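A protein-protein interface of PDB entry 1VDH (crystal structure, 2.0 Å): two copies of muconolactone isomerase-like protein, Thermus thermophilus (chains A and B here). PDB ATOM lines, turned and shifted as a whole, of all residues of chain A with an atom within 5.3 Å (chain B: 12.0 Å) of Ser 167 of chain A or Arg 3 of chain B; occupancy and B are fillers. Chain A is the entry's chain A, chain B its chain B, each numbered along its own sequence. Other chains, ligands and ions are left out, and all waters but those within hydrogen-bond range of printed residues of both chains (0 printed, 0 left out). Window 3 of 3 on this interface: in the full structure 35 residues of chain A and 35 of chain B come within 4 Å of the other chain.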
ATOM      1  N   ALA A 162     -28.288   7.035  19.106  1.00  0.00           N
ATOM      2  CA  ALA A 162     -27.755   8.387  19.246  1.00  0.00           C
ATOM      3  C   ALA A 162     -26.522   8.597  18.368  1.00  0.00           C
ATOM      4  O   ALA A 162     -26.325   9.674  17.806  1.00  0.00           O
ATOM      5  CB  ALA A 162     -27.423   8.681  20.705  1.00  0.00           C
ATOM      6  N   LYS A 163     -25.723   7.543  18.221  1.00  0.00           N
ATOM      7  CA  LYS A 163     -24.508   7.599  17.414  1.00  0.00           C
ATOM      8  C   LYS A 163     -24.799   7.922  15.945  1.00  0.00           C
ATOM      9  O   LYS A 163     -24.073   8.695  15.322  1.00  0.00           O
ATOM     10  CB  LYS A 163     -23.734   6.282  17.527  1.00  0.00           C
ATOM     11  CG  LYS A 163     -22.355   6.318  16.885  1.00  0.00           C
ATOM     12  CD  LYS A 163     -21.650   4.972  17.007  1.00  0.00           C
ATOM     13  CE  LYS A 163     -20.255   5.018  16.390  1.00  0.00           C
ATOM     14  NZ  LYS A 163     -19.348   5.957  17.112  1.00  0.00           N
ATOM     15  N   GLU A 164     -25.849   7.321  15.391  1.00  0.00           N
ATOM     16  CA  GLU A 164     -26.217   7.574  14.000  1.00  0.00           C
ATOM     17  C   GLU A 164     -26.790   8.980  13.842  1.00  0.00           C
ATOM     18  O   GLU A 164     -26.491   9.675  12.868  1.00  0.00           O
ATOM     19  CB  GLU A 164     -27.209   6.523  13.489  1.00  0.00           C
ATOM     20  CG  GLU A 164     -27.723   6.762  12.059  1.00  0.00           C
ATOM     21  CD  GLU A 164     -26.626   6.734  10.987  1.00  0.00           C
ATOM     22  OE1 GLU A 164     -25.545   6.156  11.229  1.00  0.00           O
ATOM     23  OE2 GLU A 164     -26.858   7.282   9.885  1.00  0.00           O
ATOM     24  N   ARG A 165     -27.604   9.406  14.802  1.00  0.00           N
ATOM     25  CA  ARG A 165     -28.175  10.749  14.750  1.00  0.00           C
ATOM     26  C   ARG A 165     -27.058  11.791  14.796  1.00  0.00           C
ATOM     27  O   ARG A 165     -27.118  12.808  14.101  1.00  0.00           O
ATOM     28  CB  ARG A 165     -29.170  10.964  15.893  1.00  0.00           C
ATOM     29  CG  ARG A 165     -30.529  10.315  15.631  1.00  0.00           C
ATOM     30  CD  ARG A 165     -31.533  10.623  16.727  1.00  0.00           C
ATOM     31  NE  ARG A 165     -31.582   9.576  17.746  1.00  0.00           N
ATOM     32  CZ  ARG A 165     -31.213   9.747  19.009  1.00  0.00           C
ATOM     33  NH1 ARG A 165     -30.760  10.924  19.418  1.00  0.00           N
ATOM     34  NH2 ARG A 165     -31.311   8.744  19.868  1.00  0.00           N
ATOM     35  N   ALA A 166     -26.020  11.505  15.579  1.00  0.00           N
ATOM     36  CA  ALA A 166     -24.877  12.403  15.701  1.00  0.00           C
ATOM     37  C   ALA A 166     -24.137  12.539  14.370  1.00  0.00           C
ATOM     38  O   ALA A 166     -23.776  13.645  13.970  1.00  0.00           O
ATOM     39  CB  ALA A 166     -23.924  11.906  16.789  1.00  0.00           C
ATOM     40  N   SER A 167     -23.903  11.421  13.685  1.00  0.00           N
ATOM     41  CA  SER A 167     -23.198  11.471  12.404  1.00  0.00           C
ATOM     42  C   SER A 167     -24.030  12.194  11.343  1.00  0.00           C
ATOM     43  O   SER A 167     -23.485  12.910  10.501  1.00  0.00           O
ATOM     44  CB  SER A 167     -22.806  10.069  11.924  1.00  0.00           C
ATOM     45  OG  SER A 167     -23.946   9.261  11.702  1.00  0.00           O
ATOM     46  N   LEU A 168     -25.350  12.031  11.415  1.00  0.00           N
ATOM     47  CA  LEU A 168     -26.261  12.676  10.473  1.00  0.00           C
ATOM     48  C   LEU A 168     -26.280  14.191  10.678  1.00  0.00           C
ATOM     49  O   LEU A 168     -26.296  14.954   9.709  1.00  0.00           O
ATOM     50  CB  LEU A 168     -27.670  12.087  10.615  1.00  0.00           C
ATOM     51  CG  LEU A 168     -27.829  10.658  10.081  1.00  0.00           C
ATOM     52  CD1 LEU A 168     -29.162  10.070  10.503  1.00  0.00           C
ATOM     53  CD2 LEU A 168     -27.688  10.662   8.569  1.00  0.00           C
ATOM     54  N   MET A 169     -26.247  14.623  11.938  1.00  0.00           N
ATOM     55  CA  MET A 169     -26.246  16.048  12.266  1.00  0.00           C
ATOM     56  C   MET A 169     -24.899  16.703  11.962  1.00  0.00           C
ATOM     57  O   MET A 169     -24.839  17.887  11.620  1.00  0.00           O
ATOM     58  CB  MET A 169     -26.610  16.273  13.738  1.00  0.00           C
ATOM     59  CG  MET A 169     -28.060  15.954  14.080  1.00  0.00           C
ATOM     60  SD  MET A 169     -29.252  16.869  13.064  1.00  0.00           S
ATOM     61  CE  MET A 169     -28.933  18.574  13.617  1.00  0.00           C
ATOM     62  N   LYS A 170     -23.821  15.932  12.084  1.00  0.00           N
ATOM     63  CA  LYS A 170     -22.487  16.458  11.811  1.00  0.00           C
ATOM     64  C   LYS A 170     -22.379  16.868  10.341  1.00  0.00           C
ATOM     65  O   LYS A 170     -21.904  17.962  10.029  1.00  0.00           O
ATOM     66  CB  LYS A 170     -21.407  15.432  12.176  1.00  0.00           C
ATOM     67  CG  LYS A 170     -19.995  16.004  12.160  1.00  0.00           C
ATOM     68  CD  LYS A 170     -18.974  15.032  12.732  1.00  0.00           C
ATOM     69  CE  LYS A 170     -17.581  15.658  12.757  1.00  0.00           C
ATOM     70  NZ  LYS A 170     -16.573  14.767  13.402  1.00  0.00           N
ATOM     71  N   ALA A 171     -22.870  16.007   9.451  1.00  0.00           N
ATOM     72  CA  ALA A 171     -22.847  16.272   8.012  1.00  0.00           C
ATOM     73  C   ALA A 171     -23.701  17.493   7.679  1.00  0.00           C
ATOM     74  O   ALA A 171     -23.363  18.278   6.790  1.00  0.00           O
ATOM     75  CB  ALA A 171     -23.353  15.053   7.250  1.00  0.00           C
ATOM     76  N   GLU A 221     -28.354  13.434   4.031  1.00  0.00           N
ATOM     77  CA  GLU A 221     -29.231  12.334   4.431  1.00  0.00           C
ATOM     78  C   GLU A 221     -30.225  12.700   5.532  1.00  0.00           C
ATOM     79  O   GLU A 221     -31.393  12.305   5.474  1.00  0.00           O
ATOM     80  CB  GLU A 221     -28.426  11.093   4.833  1.00  0.00           C
ATOM     81  CG  GLU A 221     -29.311   9.872   5.110  1.00  0.00           C
ATOM     82  CD  GLU A 221     -28.531   8.574   5.282  1.00  0.00           C
ATOM     83  OE1 GLU A 221     -27.318   8.539   4.984  1.00  0.00           O
ATOM     84  OE2 GLU A 221     -29.145   7.577   5.710  1.00  0.00           O
ATOM     85  N   ARG B   3     -20.200   6.251   4.161  1.00  0.00           N
ATOM     86  CA  ARG B   3     -21.502   6.942   4.388  1.00  0.00           C
ATOM     87  C   ARG B   3     -22.013   7.613   3.116  1.00  0.00           C
ATOM     88  O   ARG B   3     -21.333   7.616   2.090  1.00  0.00           O
ATOM     89  CB  ARG B   3     -21.373   7.977   5.510  1.00  0.00           C
ATOM     90  CG  ARG B   3     -21.109   7.375   6.885  1.00  0.00           C
ATOM     91  CD  ARG B   3     -21.208   8.424   7.986  1.00  0.00           C
ATOM     92  NE  ARG B   3     -22.531   9.050   8.040  1.00  0.00           N
ATOM     93  CZ  ARG B   3     -23.625   8.473   8.534  1.00  0.00           C
ATOM     94  NH1 ARG B   3     -24.776   9.132   8.534  1.00  0.00           N
ATOM     95  NH2 ARG B   3     -23.574   7.246   9.040  1.00  0.00           N
ATOM     96  N   HIS B   4     -23.213   8.178   3.195  1.00  0.00           N
ATOM     97  CA  HIS B   4     -23.827   8.852   2.055  1.00  0.00           C
ATOM     98  C   HIS B   4     -23.125  10.165   1.719  1.00  0.00           C
ATOM     99  O   HIS B   4     -22.977  11.040   2.573  1.00  0.00           O
ATOM    100  CB  HIS B   4     -25.313   9.115   2.320  1.00  0.00           C
ATOM    101  CG  HIS B   4     -26.026   9.754   1.169  1.00  0.00           C
ATOM    102  ND1 HIS B   4     -26.374   9.059   0.031  1.00  0.00           N
ATOM    103  CD2 HIS B   4     -26.438  11.029   0.971  1.00  0.00           C
ATOM    104  CE1 HIS B   4     -26.965   9.879  -0.820  1.00  0.00           C
ATOM    105  NE2 HIS B   4     -27.016  11.080  -0.274  1.00  0.00           N
ATOM    106  N   VAL B   5     -22.685  10.281   0.471  1.00  0.00           N
ATOM    107  CA  VAL B   5     -22.013  11.483  -0.001  1.00  0.00           C
ATOM    108  C   VAL B   5     -23.016  12.300  -0.816  1.00  0.00           C
ATOM    109  O   VAL B   5     -23.515  11.837  -1.845  1.00  0.00           O
ATOM    110  CB  VAL B   5     -20.797  11.141  -0.892  1.00  0.00           C
ATOM    111  CG1 VAL B   5     -20.089  12.413  -1.335  1.00  0.00           C
ATOM    112  CG2 VAL B   5     -19.834  10.231  -0.143  1.00  0.00           C
ATOM    113  N   PRO B   6     -23.368  13.502  -0.335  1.00  0.00           N
ATOM    114  CA  PRO B   6     -24.322  14.326  -1.075  1.00  0.00           C
ATOM    115  C   PRO B   6     -23.700  14.921  -2.333  1.00  0.00           C
ATOM    116  O   PRO B   6     -22.520  15.285  -2.358  1.00  0.00           O
ATOM    117  CB  PRO B   6     -24.695  15.409  -0.063  1.00  0.00           C
ATOM    118  CG  PRO B   6     -23.430  15.580   0.710  1.00  0.00           C
ATOM    119  CD  PRO B   6     -23.002  14.143   0.941  1.00  0.00           C
ATOM    120  N   GLU B   7     -24.505  14.972  -3.385  1.00  0.00           N
ATOM    121  CA  GLU B   7     -24.098  15.522  -4.666  1.00  0.00           C
ATOM    122  C   GLU B   7     -25.203  16.504  -5.021  1.00  0.00           C
ATOM    123  O   GLU B   7     -25.997  16.256  -5.926  1.00  0.00           O
ATOM    124  CB  GLU B   7     -24.034  14.409  -5.715  1.00  0.00           C
ATOM    125  CG  GLU B   7     -22.744  14.398  -6.512  1.00  0.00           C
ATOM    126  CD  GLU B   7     -21.531  14.135  -5.642  1.00  0.00           C
ATOM    127  OE1 GLU B   7     -20.509  14.836  -5.819  1.00  0.00           O
ATOM    128  OE2 GLU B   7     -21.603  13.230  -4.779  1.00  0.00           O
ATOM    129  N   TYR B 158     -33.940  12.974  -3.481  1.00  0.00           N
ATOM    130  CA  TYR B 158     -32.779  13.565  -2.836  1.00  0.00           C
ATOM    131  C   TYR B 158     -31.677  12.614  -2.367  1.00  0.00           C
ATOM    132  O   TYR B 158     -30.558  13.054  -2.119  1.00  0.00           O
ATOM    133  CB  TYR B 158     -33.230  14.513  -1.722  1.00  0.00           C
ATOM    134  CG  TYR B 158     -33.951  15.741  -2.263  1.00  0.00           C
ATOM    135  CD1 TYR B 158     -33.255  16.917  -2.549  1.00  0.00           C
ATOM    136  CD2 TYR B 158     -35.322  15.715  -2.510  1.00  0.00           C
ATOM    137  CE1 TYR B 158     -33.912  18.040  -3.071  1.00  0.00           C
ATOM    138  CE2 TYR B 158     -35.985  16.823  -3.026  1.00  0.00           C
ATOM    139  CZ  TYR B 158     -35.278  17.981  -3.306  1.00  0.00           C
ATOM    140  OH  TYR B 158     -35.944  19.068  -3.826  1.00  0.00           O
ATOM    141  N   MET B 159     -31.983  11.320  -2.263  1.00  0.00           N
ATOM    142  CA  MET B 159     -30.986  10.322  -1.857  1.00  0.00           C
ATOM    143  C   MET B 159     -30.288   9.666  -3.057  1.00  0.00           C
ATOM    144  O   MET B 159     -29.293   8.952  -2.897  1.00  0.00           O
ATOM    145  CB  MET B 159     -31.628   9.233  -0.989  1.00  0.00           C
ATOM    146  CG  MET B 159     -31.920   9.666   0.441  1.00  0.00           C
ATOM    147  SD  MET B 159     -30.399  10.057   1.331  1.00  0.00           S
ATOM    148  CE  MET B 159     -29.680   8.397   1.490  1.00  0.00           C
ATOM    149  N   LEU B 160     -30.823   9.892  -4.253  1.00  0.00           N
ATOM    150  CA  LEU B 160     -30.257   9.324  -5.476  1.00  0.00           C
ATOM    151  C   LEU B 160     -28.906   9.928  -5.840  1.00  0.00           C
ATOM    152  O   LEU B 160     -28.590  11.051  -5.449  1.00  0.00           O
ATOM    153  CB  LEU B 160     -31.191   9.573  -6.668  1.00  0.00           C
ATOM    154  CG  LEU B 160     -32.565   8.914  -6.799  1.00  0.00           C
ATOM    155  CD1 LEU B 160     -33.252   9.474  -8.040  1.00  0.00           C
ATOM    156  CD2 LEU B 160     -32.419   7.398  -6.906  1.00  0.00           C
ATOM    157  N   PRO B 161     -28.072   9.164  -6.567  1.00  0.00           N
ATOM    158  CA  PRO B 161     -26.755   9.659  -6.994  1.00  0.00           C
ATOM    159  C   PRO B 161     -27.019  10.714  -8.078  1.00  0.00           C
ATOM    160  O   PRO B 161     -28.030  10.632  -8.789  1.00  0.00           O
ATOM    161  CB  PRO B 161     -26.107   8.413  -7.612  1.00  0.00           C
ATOM    162  CG  PRO B 161     -26.771   7.271  -6.886  1.00  0.00           C
ATOM    163  CD  PRO B 161     -28.206   7.719  -6.829  1.00  0.00           C
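The guanidinium group (NH1) of Arg 3 of chain B lies within salt-bridge range of the side-chain carboxylate (OE2) of Glu 164 of chain A (3.1 Å).
The guanidinium group of Arg 3 of chain B sits at hydrogen-bond distance from the side-chain hydroxyl of Ser 167 of chain A (3.3 Å).
The backbone carbonyl oxygen (O) of Glu 164 of chain A is in hydrogen-bond range of the side-chain hydroxyl (OG) of Ser 167 of chain A (2.8 Å).
Among the printed residues, merely in contact across the chains: Leu 168 of chain A with Arg 3 of chain B (3.3 Å), Glu 221 of chain A with His 4 of chain B (3.4 Å) and Glu 221 of chain A with Met 159 of chain B (3.9 Å).
Of chain B, only Arg 3 (3.3 Å) comes within 4 Å of Ser 167 of chain A.
Arg 3 of chain B touches three residues of chain A.
Lys 163 of chain A touches none of the printed residues of chain B.
Of chain B, only Arg 3 (3.1 Å) comes within 4 Å of Glu 164 of chain A.
No residue of chain B comes within 4 Å of Ala 166 of chain A.
No residue of chain B comes within 4 Å of Lys 170 of chain A.
No residue of chain B comes within 4 Å of Ala 171 of chain A.
Printed residues of chain A within 4 Å of Met 159 of chain B: Glu 221 (3.9 Å).
Printed residues of chain A within 4 Å of His 4 of chain B: Glu 221.
Of the printed residues of chain B, Glu 221 of chain A touches His 4 (3.4 Å) and Met 159 (3.9 Å).
Tyr 158 of chain B touches none of the printed residues of chain A.
The nearest residue of chain B that does not touch Ser 167 of chain A is His 4 of chain B (8.2 Å).
Of the 9 printed residues of chain B, 3 touch a printed residue of chain A.
Printed residues of chain B that touch a printed residue of chain A: Arg 3, His 4 and Met 159.
Hydrophobic or aromatic side chains of chain B within 4 Å of the printed part of chain A: His 4 and Met 159.
Of the 11 printed residues of chain A, 4 touch a printed residue of chain B.
Among the printed residues, Asp or Glu carboxylates within 4 Å of a Lys or Arg side-chain nitrogen of the other chain: Glu 164 of chain A with Arg 3 of chain B (3.1 Å).
No position is printed for both chains.
Of the 5 pairs that touch across the chains among the printed residues, none has its exchanged pair printed and touching as well.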
